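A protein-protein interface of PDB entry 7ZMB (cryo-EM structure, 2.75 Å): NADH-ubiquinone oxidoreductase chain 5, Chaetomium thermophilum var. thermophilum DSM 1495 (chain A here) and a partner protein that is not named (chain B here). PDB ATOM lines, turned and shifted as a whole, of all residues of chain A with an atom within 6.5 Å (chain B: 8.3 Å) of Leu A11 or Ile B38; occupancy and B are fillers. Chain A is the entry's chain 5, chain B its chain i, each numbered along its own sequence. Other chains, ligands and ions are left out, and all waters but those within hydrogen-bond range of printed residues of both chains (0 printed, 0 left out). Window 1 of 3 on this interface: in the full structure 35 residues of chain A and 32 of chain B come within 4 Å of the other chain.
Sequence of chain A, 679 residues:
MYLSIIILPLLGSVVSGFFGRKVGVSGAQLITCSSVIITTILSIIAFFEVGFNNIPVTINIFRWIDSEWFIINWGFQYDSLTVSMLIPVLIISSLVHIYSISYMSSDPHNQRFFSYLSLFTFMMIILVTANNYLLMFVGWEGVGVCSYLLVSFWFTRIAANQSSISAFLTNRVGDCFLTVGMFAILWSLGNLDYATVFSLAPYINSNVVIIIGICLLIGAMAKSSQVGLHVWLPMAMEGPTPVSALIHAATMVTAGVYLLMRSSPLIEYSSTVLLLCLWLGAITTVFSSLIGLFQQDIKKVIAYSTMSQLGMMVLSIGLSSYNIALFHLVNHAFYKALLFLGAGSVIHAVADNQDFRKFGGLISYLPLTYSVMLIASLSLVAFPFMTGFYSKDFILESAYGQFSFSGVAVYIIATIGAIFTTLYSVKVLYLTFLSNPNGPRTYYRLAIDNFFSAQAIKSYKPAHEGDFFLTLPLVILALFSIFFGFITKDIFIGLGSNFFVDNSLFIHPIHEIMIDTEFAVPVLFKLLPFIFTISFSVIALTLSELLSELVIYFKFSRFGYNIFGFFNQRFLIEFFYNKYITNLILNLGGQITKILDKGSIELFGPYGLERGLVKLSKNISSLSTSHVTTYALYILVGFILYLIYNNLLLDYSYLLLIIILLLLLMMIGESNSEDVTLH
O of Ile B38 sits at hydrogen-bond distance from OG1 of Thr B42 (2.4 Å).
The side-chain hydroxyl (OG) of Ser A35 is in hydrogen-bond range of the backbone carbonyl oxygen (O) of Ile A31.
Among the printed residues, pairs that only touch across the chains: Ile A7 with Val B45, Leu A8 with Ile B38, Leu A8 with Thr B42, Leu A11 with Ile B38, Leu A11 with Ile B41, Val A15 with Phe B34, Ile A31 with Thr B31 and Ile A31 with Ile B38.
Of the printed residues of chain B, Ile A7 touches Val B45.
Of the printed residues of chain B, Leu A8 touches Ile B38 and Thr B42.
Printed residues of chain B within 4 Å of Leu A11: Ile B38 and Ile B41.
No residue of chain B comes within 4 Å of Gly A12.
Printed residues of chain B within 4 Å of Val A15: Phe B34.
Ile B38 touches three residues of chain A.
Printed residues of chain A within 4 Å of Ile B41: Leu A11.
Printed residues of chain A within 4 Å of Thr B42: Leu A8 (3.3 Å).
The nearest printed residue of chain A that does not touch Thr B42 is Leu A11 (4.1 Å).
Of the 15 printed residues of chain B, 6 touch a printed residue of chain A.
Printed residues of chain B that touch a printed residue of chain A: Thr B31, Phe B34, Ile B38, Ile B41, Thr B42 and Val B45.
Of the 14 printed residues of chain A, 5 touch a printed residue of chain B.
Among the printed residues, no Asp or Glu carboxylate lies within 4 Å of a Lys or Arg side-chain nitrogen of the other chain.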
ATOM      1  N   ILE A   6      27.072 -39.161 -22.376  1.00  0.00           N
ATOM      2  CA  ILE A   6      25.771 -38.956 -22.987  1.00  0.00           C
ATOM      3  C   ILE A   6      25.470 -37.474 -23.177  1.00  0.00           C
ATOM      4  O   ILE A   6      24.813 -37.089 -24.142  1.00  0.00           O
ATOM      5  CB  ILE A   6      24.683 -39.647 -22.135  1.00  0.00           C
ATOM      6  CG1 ILE A   6      24.677 -41.152 -22.381  1.00  0.00           C
ATOM      7  CG2 ILE A   6      23.301 -39.059 -22.403  1.00  0.00           C
ATOM      8  CD1 ILE A   6      24.218 -41.945 -21.193  1.00  0.00           C
ATOM      9  N   ILE A   7      25.975 -36.623 -22.288  1.00  0.00           N
ATOM     10  CA  ILE A   7      25.552 -35.229 -22.275  1.00  0.00           C
ATOM     11  C   ILE A   7      26.404 -34.387 -23.213  1.00  0.00           C
ATOM     12  O   ILE A   7      25.880 -33.535 -23.939  1.00  0.00           O
ATOM     13  CB  ILE A   7      25.579 -34.678 -20.839  1.00  0.00           C
ATOM     14  CG1 ILE A   7      24.658 -35.502 -19.945  1.00  0.00           C
ATOM     15  CG2 ILE A   7      25.130 -33.235 -20.820  1.00  0.00           C
ATOM     16  CD1 ILE A   7      23.212 -35.477 -20.377  1.00  0.00           C
ATOM     17  N   LEU A   8      27.719 -34.603 -23.217  1.00  0.00           N
ATOM     18  CA  LEU A   8      28.633 -33.745 -23.970  1.00  0.00           C
ATOM     19  C   LEU A   8      28.258 -33.592 -25.441  1.00  0.00           C
ATOM     20  O   LEU A   8      28.161 -32.454 -25.916  1.00  0.00           O
ATOM     21  CB  LEU A   8      30.077 -34.251 -23.866  1.00  0.00           C
ATOM     22  CG  LEU A   8      30.923 -33.869 -22.651  1.00  0.00           C
ATOM     23  CD1 LEU A   8      31.135 -32.367 -22.627  1.00  0.00           C
ATOM     24  CD2 LEU A   8      30.297 -34.332 -21.359  1.00  0.00           C
ATOM     25  N   PRO A   9      28.034 -34.677 -26.199  1.00  0.00           N
ATOM     26  CA  PRO A   9      27.677 -34.489 -27.612  1.00  0.00           C
ATOM     27  C   PRO A   9      26.398 -33.697 -27.795  1.00  0.00           C
ATOM     28  O   PRO A   9      26.269 -32.967 -28.784  1.00  0.00           O
ATOM     29  CB  PRO A   9      27.545 -35.924 -28.137  1.00  0.00           C
ATOM     30  CG  PRO A   9      28.262 -36.760 -27.158  1.00  0.00           C
ATOM     31  CD  PRO A   9      28.056 -36.106 -25.847  1.00  0.00           C
ATOM     32  N   LEU A  10      25.452 -33.813 -26.864  1.00  0.00           N
ATOM     33  CA  LEU A  10      24.267 -32.965 -26.895  1.00  0.00           C
ATOM     34  C   LEU A  10      24.620 -31.500 -26.690  1.00  0.00           C
ATOM     35  O   LEU A  10      24.036 -30.630 -27.340  1.00  0.00           O
ATOM     36  CB  LEU A  10      23.266 -33.423 -25.834  1.00  0.00           C
ATOM     37  CG  LEU A  10      21.873 -32.784 -25.801  1.00  0.00           C
ATOM     38  CD1 LEU A  10      20.879 -33.741 -25.200  1.00  0.00           C
ATOM     39  CD2 LEU A  10      21.851 -31.479 -25.013  1.00  0.00           C
ATOM     40  N   LEU A  11      25.557 -31.206 -25.787  1.00  0.00           N
ATOM     41  CA  LEU A  11      25.829 -29.819 -25.431  1.00  0.00           C
ATOM     42  C   LEU A  11      26.529 -29.074 -26.559  1.00  0.00           C
ATOM     43  O   LEU A  11      26.224 -27.906 -26.817  1.00  0.00           O
ATOM     44  CB  LEU A  11      26.671 -29.758 -24.164  1.00  0.00           C
ATOM     45  CG  LEU A  11      25.984 -30.272 -22.911  1.00  0.00           C
ATOM     46  CD1 LEU A  11      26.973 -30.281 -21.762  1.00  0.00           C
ATOM     47  CD2 LEU A  11      24.760 -29.435 -22.594  1.00  0.00           C
ATOM     48  N   GLY A  12      27.475 -29.729 -27.228  1.00  0.00           N
ATOM     49  CA  GLY A  12      28.099 -29.114 -28.384  1.00  0.00           C
ATOM     50  C   GLY A  12      27.099 -28.764 -29.469  1.00  0.00           C
ATOM     51  O   GLY A  12      27.206 -27.714 -30.103  1.00  0.00           O
ATOM     52  N   SER A  13      26.093 -29.624 -29.674  1.00  0.00           N
ATOM     53  CA  SER A  13      25.183 -29.447 -30.801  1.00  0.00           C
ATOM     54  C   SER A  13      24.253 -28.250 -30.608  1.00  0.00           C
ATOM     55  O   SER A  13      23.947 -27.539 -31.570  1.00  0.00           O
ATOM     56  CB  SER A  13      24.375 -30.725 -31.035  1.00  0.00           C
ATOM     57  OG  SER A  13      23.805 -31.207 -29.837  1.00  0.00           O
ATOM     58  N   VAL A  14      23.778 -28.017 -29.386  1.00  0.00           N
ATOM     59  CA  VAL A  14      22.856 -26.907 -29.174  1.00  0.00           C
ATOM     60  C   VAL A  14      23.587 -25.577 -29.304  1.00  0.00           C
ATOM     61  O   VAL A  14      23.055 -24.612 -29.865  1.00  0.00           O
ATOM     62  CB  VAL A  14      22.141 -27.048 -27.817  1.00  0.00           C
ATOM     63  CG1 VAL A  14      21.331 -28.328 -27.787  1.00  0.00           C
ATOM     64  CG2 VAL A  14      23.128 -27.038 -26.668  1.00  0.00           C
ATOM     65  N   VAL A  15      24.819 -25.504 -28.798  1.00  0.00           N
ATOM     66  CA  VAL A  15      25.617 -24.299 -28.965  1.00  0.00           C
ATOM     67  C   VAL A  15      26.002 -24.126 -30.427  1.00  0.00           C
ATOM     68  O   VAL A  15      26.029 -23.006 -30.949  1.00  0.00           O
ATOM     69  CB  VAL A  15      26.850 -24.351 -28.046  1.00  0.00           C
ATOM     70  CG1 VAL A  15      27.747 -23.146 -28.272  1.00  0.00           C
ATOM     71  CG2 VAL A  15      26.417 -24.431 -26.601  1.00  0.00           C
ATOM     72  N   SER A  16      26.303 -25.227 -31.111  1.00  0.00           N
ATOM     73  CA  SER A  16      26.600 -25.154 -32.535  1.00  0.00           C
ATOM     74  C   SER A  16      25.376 -24.736 -33.341  1.00  0.00           C
ATOM     75  O   SER A  16      25.493 -23.983 -34.309  1.00  0.00           O
ATOM     76  CB  SER A  16      27.132 -26.499 -33.026  1.00  0.00           C
ATOM     77  OG  SER A  16      27.834 -26.356 -34.243  1.00  0.00           O
ATOM     78  N   ILE A  31      34.137 -26.306 -30.576  1.00  0.00           N
ATOM     79  CA  ILE A  31      33.316 -26.782 -29.466  1.00  0.00           C
ATOM     80  C   ILE A  31      32.862 -28.216 -29.708  1.00  0.00           C
ATOM     81  O   ILE A  31      33.013 -29.090 -28.847  1.00  0.00           O
ATOM     82  CB  ILE A  31      32.114 -25.846 -29.250  1.00  0.00           C
ATOM     83  CG1 ILE A  31      32.571 -24.504 -28.680  1.00  0.00           C
ATOM     84  CG2 ILE A  31      31.074 -26.508 -28.366  1.00  0.00           C
ATOM     85  CD1 ILE A  31      33.226 -24.617 -27.326  1.00  0.00           C
ATOM     86  N   THR A  32      32.304 -28.480 -30.885  1.00  0.00           N
ATOM     87  CA  THR A  32      31.695 -29.781 -31.126  1.00  0.00           C
ATOM     88  C   THR A  32      32.744 -30.868 -31.291  1.00  0.00           C
ATOM     89  O   THR A  32      32.573 -31.981 -30.785  1.00  0.00           O
ATOM     90  CB  THR A  32      30.783 -29.713 -32.348  1.00  0.00           C
ATOM     91  OG1 THR A  32      31.527 -29.264 -33.484  1.00  0.00           O
ATOM     92  CG2 THR A  32      29.659 -28.759 -32.089  1.00  0.00           C
ATOM     93  N   SER A  35      34.063 -31.682 -27.887  1.00  0.00           N
ATOM     94  CA  SER A  35      33.068 -32.468 -27.173  1.00  0.00           C
ATOM     95  C   SER A  35      33.093 -33.912 -27.637  1.00  0.00           C
ATOM     96  O   SER A  35      33.015 -34.837 -26.823  1.00  0.00           O
ATOM     97  CB  SER A  35      31.677 -31.863 -27.371  1.00  0.00           C
ATOM     98  OG  SER A  35      31.573 -30.594 -26.747  1.00  0.00           O
ATOM     99  N   THR B  31      33.279 -18.042 -27.570  1.00  0.00           N
ATOM    100  CA  THR B  31      33.555 -19.473 -27.511  1.00  0.00           C
ATOM    101  C   THR B  31      34.040 -19.866 -26.126  1.00  0.00           C
ATOM    102  O   THR B  31      33.615 -20.888 -25.575  1.00  0.00           O
ATOM    103  CB  THR B  31      34.588 -19.867 -28.567  1.00  0.00           C
ATOM    104  OG1 THR B  31      34.061 -19.622 -29.877  1.00  0.00           O
ATOM    105  CG2 THR B  31      34.947 -21.340 -28.439  1.00  0.00           C
ATOM    106  N   ALA B  32      34.926 -19.058 -25.542  1.00  0.00           N
ATOM    107  CA  ALA B  32      35.370 -19.315 -24.178  1.00  0.00           C
ATOM    108  C   ALA B  32      34.210 -19.220 -23.198  1.00  0.00           C
ATOM    109  O   ALA B  32      34.104 -20.029 -22.271  1.00  0.00           O
ATOM    110  CB  ALA B  32      36.482 -18.340 -23.795  1.00  0.00           C
ATOM    111  N   ILE B  33      33.327 -18.239 -23.389  1.00  0.00           N
ATOM    112  CA  ILE B  33      32.187 -18.077 -22.489  1.00  0.00           C
ATOM    113  C   ILE B  33      31.291 -19.305 -22.544  1.00  0.00           C
ATOM    114  O   ILE B  33      30.870 -19.836 -21.512  1.00  0.00           O
ATOM    115  CB  ILE B  33      31.413 -16.792 -22.827  1.00  0.00           C
ATOM    116  CG1 ILE B  33      32.134 -15.573 -22.251  1.00  0.00           C
ATOM    117  CG2 ILE B  33      29.992 -16.868 -22.297  1.00  0.00           C
ATOM    118  CD1 ILE B  33      31.379 -14.275 -22.431  1.00  0.00           C
ATOM    119  N   PHE B  34      30.992 -19.782 -23.752  1.00  0.00           N
ATOM    120  CA  PHE B  34      30.189 -20.993 -23.881  1.00  0.00           C
ATOM    121  C   PHE B  34      30.943 -22.224 -23.401  1.00  0.00           C
ATOM    122  O   PHE B  34      30.340 -23.123 -22.805  1.00  0.00           O
ATOM    123  CB  PHE B  34      29.743 -21.176 -25.331  1.00  0.00           C
ATOM    124  CG  PHE B  34      28.531 -20.378 -25.693  1.00  0.00           C
ATOM    125  CD1 PHE B  34      28.653 -19.076 -26.139  1.00  0.00           C
ATOM    126  CD2 PHE B  34      27.271 -20.924 -25.576  1.00  0.00           C
ATOM    127  CE1 PHE B  34      27.537 -18.336 -26.467  1.00  0.00           C
ATOM    128  CE2 PHE B  34      26.155 -20.194 -25.901  1.00  0.00           C
ATOM    129  CZ  PHE B  34      26.285 -18.899 -26.345  1.00  0.00           C
ATOM    130  N   GLY B  35      32.254 -22.283 -23.646  1.00  0.00           N
ATOM    131  CA  GLY B  35      33.034 -23.435 -23.228  1.00  0.00           C
ATOM    132  C   GLY B  35      33.040 -23.644 -21.730  1.00  0.00           C
ATOM    133  O   GLY B  35      33.094 -24.782 -21.259  1.00  0.00           O
ATOM    134  N   LEU B  36      33.002 -22.557 -20.959  1.00  0.00           N
ATOM    135  CA  LEU B  36      32.875 -22.689 -19.513  1.00  0.00           C
ATOM    136  C   LEU B  36      31.545 -23.328 -19.139  1.00  0.00           C
ATOM    137  O   LEU B  36      31.474 -24.123 -18.195  1.00  0.00           O
ATOM    138  CB  LEU B  36      33.026 -21.324 -18.842  1.00  0.00           C
ATOM    139  CG  LEU B  36      34.426 -20.915 -18.370  1.00  0.00           C
ATOM    140  CD1 LEU B  36      34.881 -21.810 -17.230  1.00  0.00           C
ATOM    141  CD2 LEU B  36      35.434 -20.947 -19.508  1.00  0.00           C
ATOM    142  N   VAL B  37      30.480 -22.995 -19.870  1.00  0.00           N
ATOM    143  CA  VAL B  37      29.166 -23.552 -19.569  1.00  0.00           C
ATOM    144  C   VAL B  37      29.166 -25.060 -19.766  1.00  0.00           C
ATOM    145  O   VAL B  37      28.614 -25.806 -18.950  1.00  0.00           O
ATOM    146  CB  VAL B  37      28.083 -22.874 -20.425  1.00  0.00           C
ATOM    147  CG1 VAL B  37      26.705 -23.221 -19.895  1.00  0.00           C
ATOM    148  CG2 VAL B  37      28.285 -21.370 -20.436  1.00  0.00           C
ATOM    149  N   ILE B  38      29.769 -25.534 -20.860  1.00  0.00           N
ATOM    150  CA  ILE B  38      29.792 -26.970 -21.121  1.00  0.00           C
ATOM    151  C   ILE B  38      30.569 -27.690 -20.033  1.00  0.00           C
ATOM    152  O   ILE B  38      30.120 -28.706 -19.497  1.00  0.00           O
ATOM    153  CB  ILE B  38      30.369 -27.261 -22.513  1.00  0.00           C
ATOM    154  CG1 ILE B  38      29.482 -26.658 -23.591  1.00  0.00           C
ATOM    155  CG2 ILE B  38      30.490 -28.750 -22.728  1.00  0.00           C
ATOM    156  CD1 ILE B  38      30.108 -26.682 -24.946  1.00  0.00           C
ATOM    157  N   PHE B  39      31.737 -27.159 -19.675  1.00  0.00           N
ATOM    158  CA  PHE B  39      32.497 -27.728 -18.568  1.00  0.00           C
ATOM    159  C   PHE B  39      31.715 -27.642 -17.265  1.00  0.00           C
ATOM    160  O   PHE B  39      31.686 -28.601 -16.487  1.00  0.00           O
ATOM    161  CB  PHE B  39      33.841 -27.006 -18.439  1.00  0.00           C
ATOM    162  CG  PHE B  39      34.755 -27.587 -17.394  1.00  0.00           C
ATOM    163  CD1 PHE B  39      34.597 -27.273 -16.054  1.00  0.00           C
ATOM    164  CD2 PHE B  39      35.800 -28.417 -17.761  1.00  0.00           C
ATOM    165  CE1 PHE B  39      35.445 -27.797 -15.098  1.00  0.00           C
ATOM    166  CE2 PHE B  39      36.652 -28.946 -16.809  1.00  0.00           C
ATOM    167  CZ  PHE B  39      36.475 -28.634 -15.476  1.00  0.00           C
ATOM    168  N   GLY B  40      31.073 -26.500 -17.015  1.00  0.00           N
ATOM    169  CA  GLY B  40      30.404 -26.304 -15.740  1.00  0.00           C
ATOM    170  C   GLY B  40      29.343 -27.351 -15.470  1.00  0.00           C
ATOM    171  O   GLY B  40      29.279 -27.923 -14.379  1.00  0.00           O
ATOM    172  N   ILE B  41      28.507 -27.632 -16.468  1.00  0.00           N
ATOM    173  CA  ILE B  41      27.454 -28.616 -16.262  1.00  0.00           C
ATOM    174  C   ILE B  41      27.917 -30.033 -16.567  1.00  0.00           C
ATOM    175  O   ILE B  41      27.225 -30.988 -16.207  1.00  0.00           O
ATOM    176  CB  ILE B  41      26.207 -28.245 -17.078  1.00  0.00           C
ATOM    177  CG1 ILE B  41      26.415 -28.517 -18.561  1.00  0.00           C
ATOM    178  CG2 ILE B  41      25.849 -26.786 -16.863  1.00  0.00           C
ATOM    179  CD1 ILE B  41      25.211 -28.154 -19.379  1.00  0.00           C
ATOM    180  N   THR B  42      29.068 -30.205 -17.212  1.00  0.00           N
ATOM    181  CA  THR B  42      29.604 -31.547 -17.402  1.00  0.00           C
ATOM    182  C   THR B  42      30.018 -32.165 -16.076  1.00  0.00           C
ATOM    183  O   THR B  42      29.618 -33.289 -15.750  1.00  0.00           O
ATOM    184  CB  THR B  42      30.792 -31.508 -18.363  1.00  0.00           C
ATOM    185  OG1 THR B  42      30.339 -31.138 -19.671  1.00  0.00           O
ATOM    186  CG2 THR B  42      31.491 -32.857 -18.408  1.00  0.00           C
ATOM    187  N   ALA B  43      30.827 -31.447 -15.295  1.00  0.00           N
ATOM    188  CA  ALA B  43      31.160 -31.922 -13.959  1.00  0.00           C
ATOM    189  C   ALA B  43      29.915 -31.973 -13.092  1.00  0.00           C
ATOM    190  O   ALA B  43      29.799 -32.821 -12.199  1.00  0.00           O
ATOM    191  CB  ALA B  43      32.226 -31.027 -13.329  1.00  0.00           C
ATOM    192  N   MET B  44      28.971 -31.065 -13.346  1.00  0.00           N
ATOM    193  CA  MET B  44      27.672 -31.131 -12.695  1.00  0.00           C
ATOM    194  C   MET B  44      26.988 -32.450 -13.012  1.00  0.00           C
ATOM    195  O   MET B  44      26.429 -33.104 -12.124  1.00  0.00           O
ATOM    196  CB  MET B  44      26.825 -29.954 -13.160  1.00  0.00           C
ATOM    197  CG  MET B  44      25.633 -29.610 -12.320  1.00  0.00           C
ATOM    198  SD  MET B  44      25.438 -27.826 -12.437  1.00  0.00           S
ATOM    199  CE  MET B  44      24.324 -27.524 -11.091  1.00  0.00           C
ATOM    200  N   VAL B  45      27.022 -32.857 -14.278  1.00  0.00           N
ATOM    201  CA  VAL B  45      26.614 -34.210 -14.642  1.00  0.00           C
ATOM    202  C   VAL B  45      27.537 -35.239 -13.999  1.00  0.00           C
ATOM    203  O   VAL B  45      27.081 -36.242 -13.438  1.00  0.00           O
ATOM    204  CB  VAL B  45      26.583 -34.362 -16.169  1.00  0.00           C
ATOM    205  CG1 VAL B  45      26.348 -35.802 -16.525  1.00  0.00           C
ATOM    206  CG2 VAL B  45      25.488 -33.499 -16.752  1.00  0.00           C
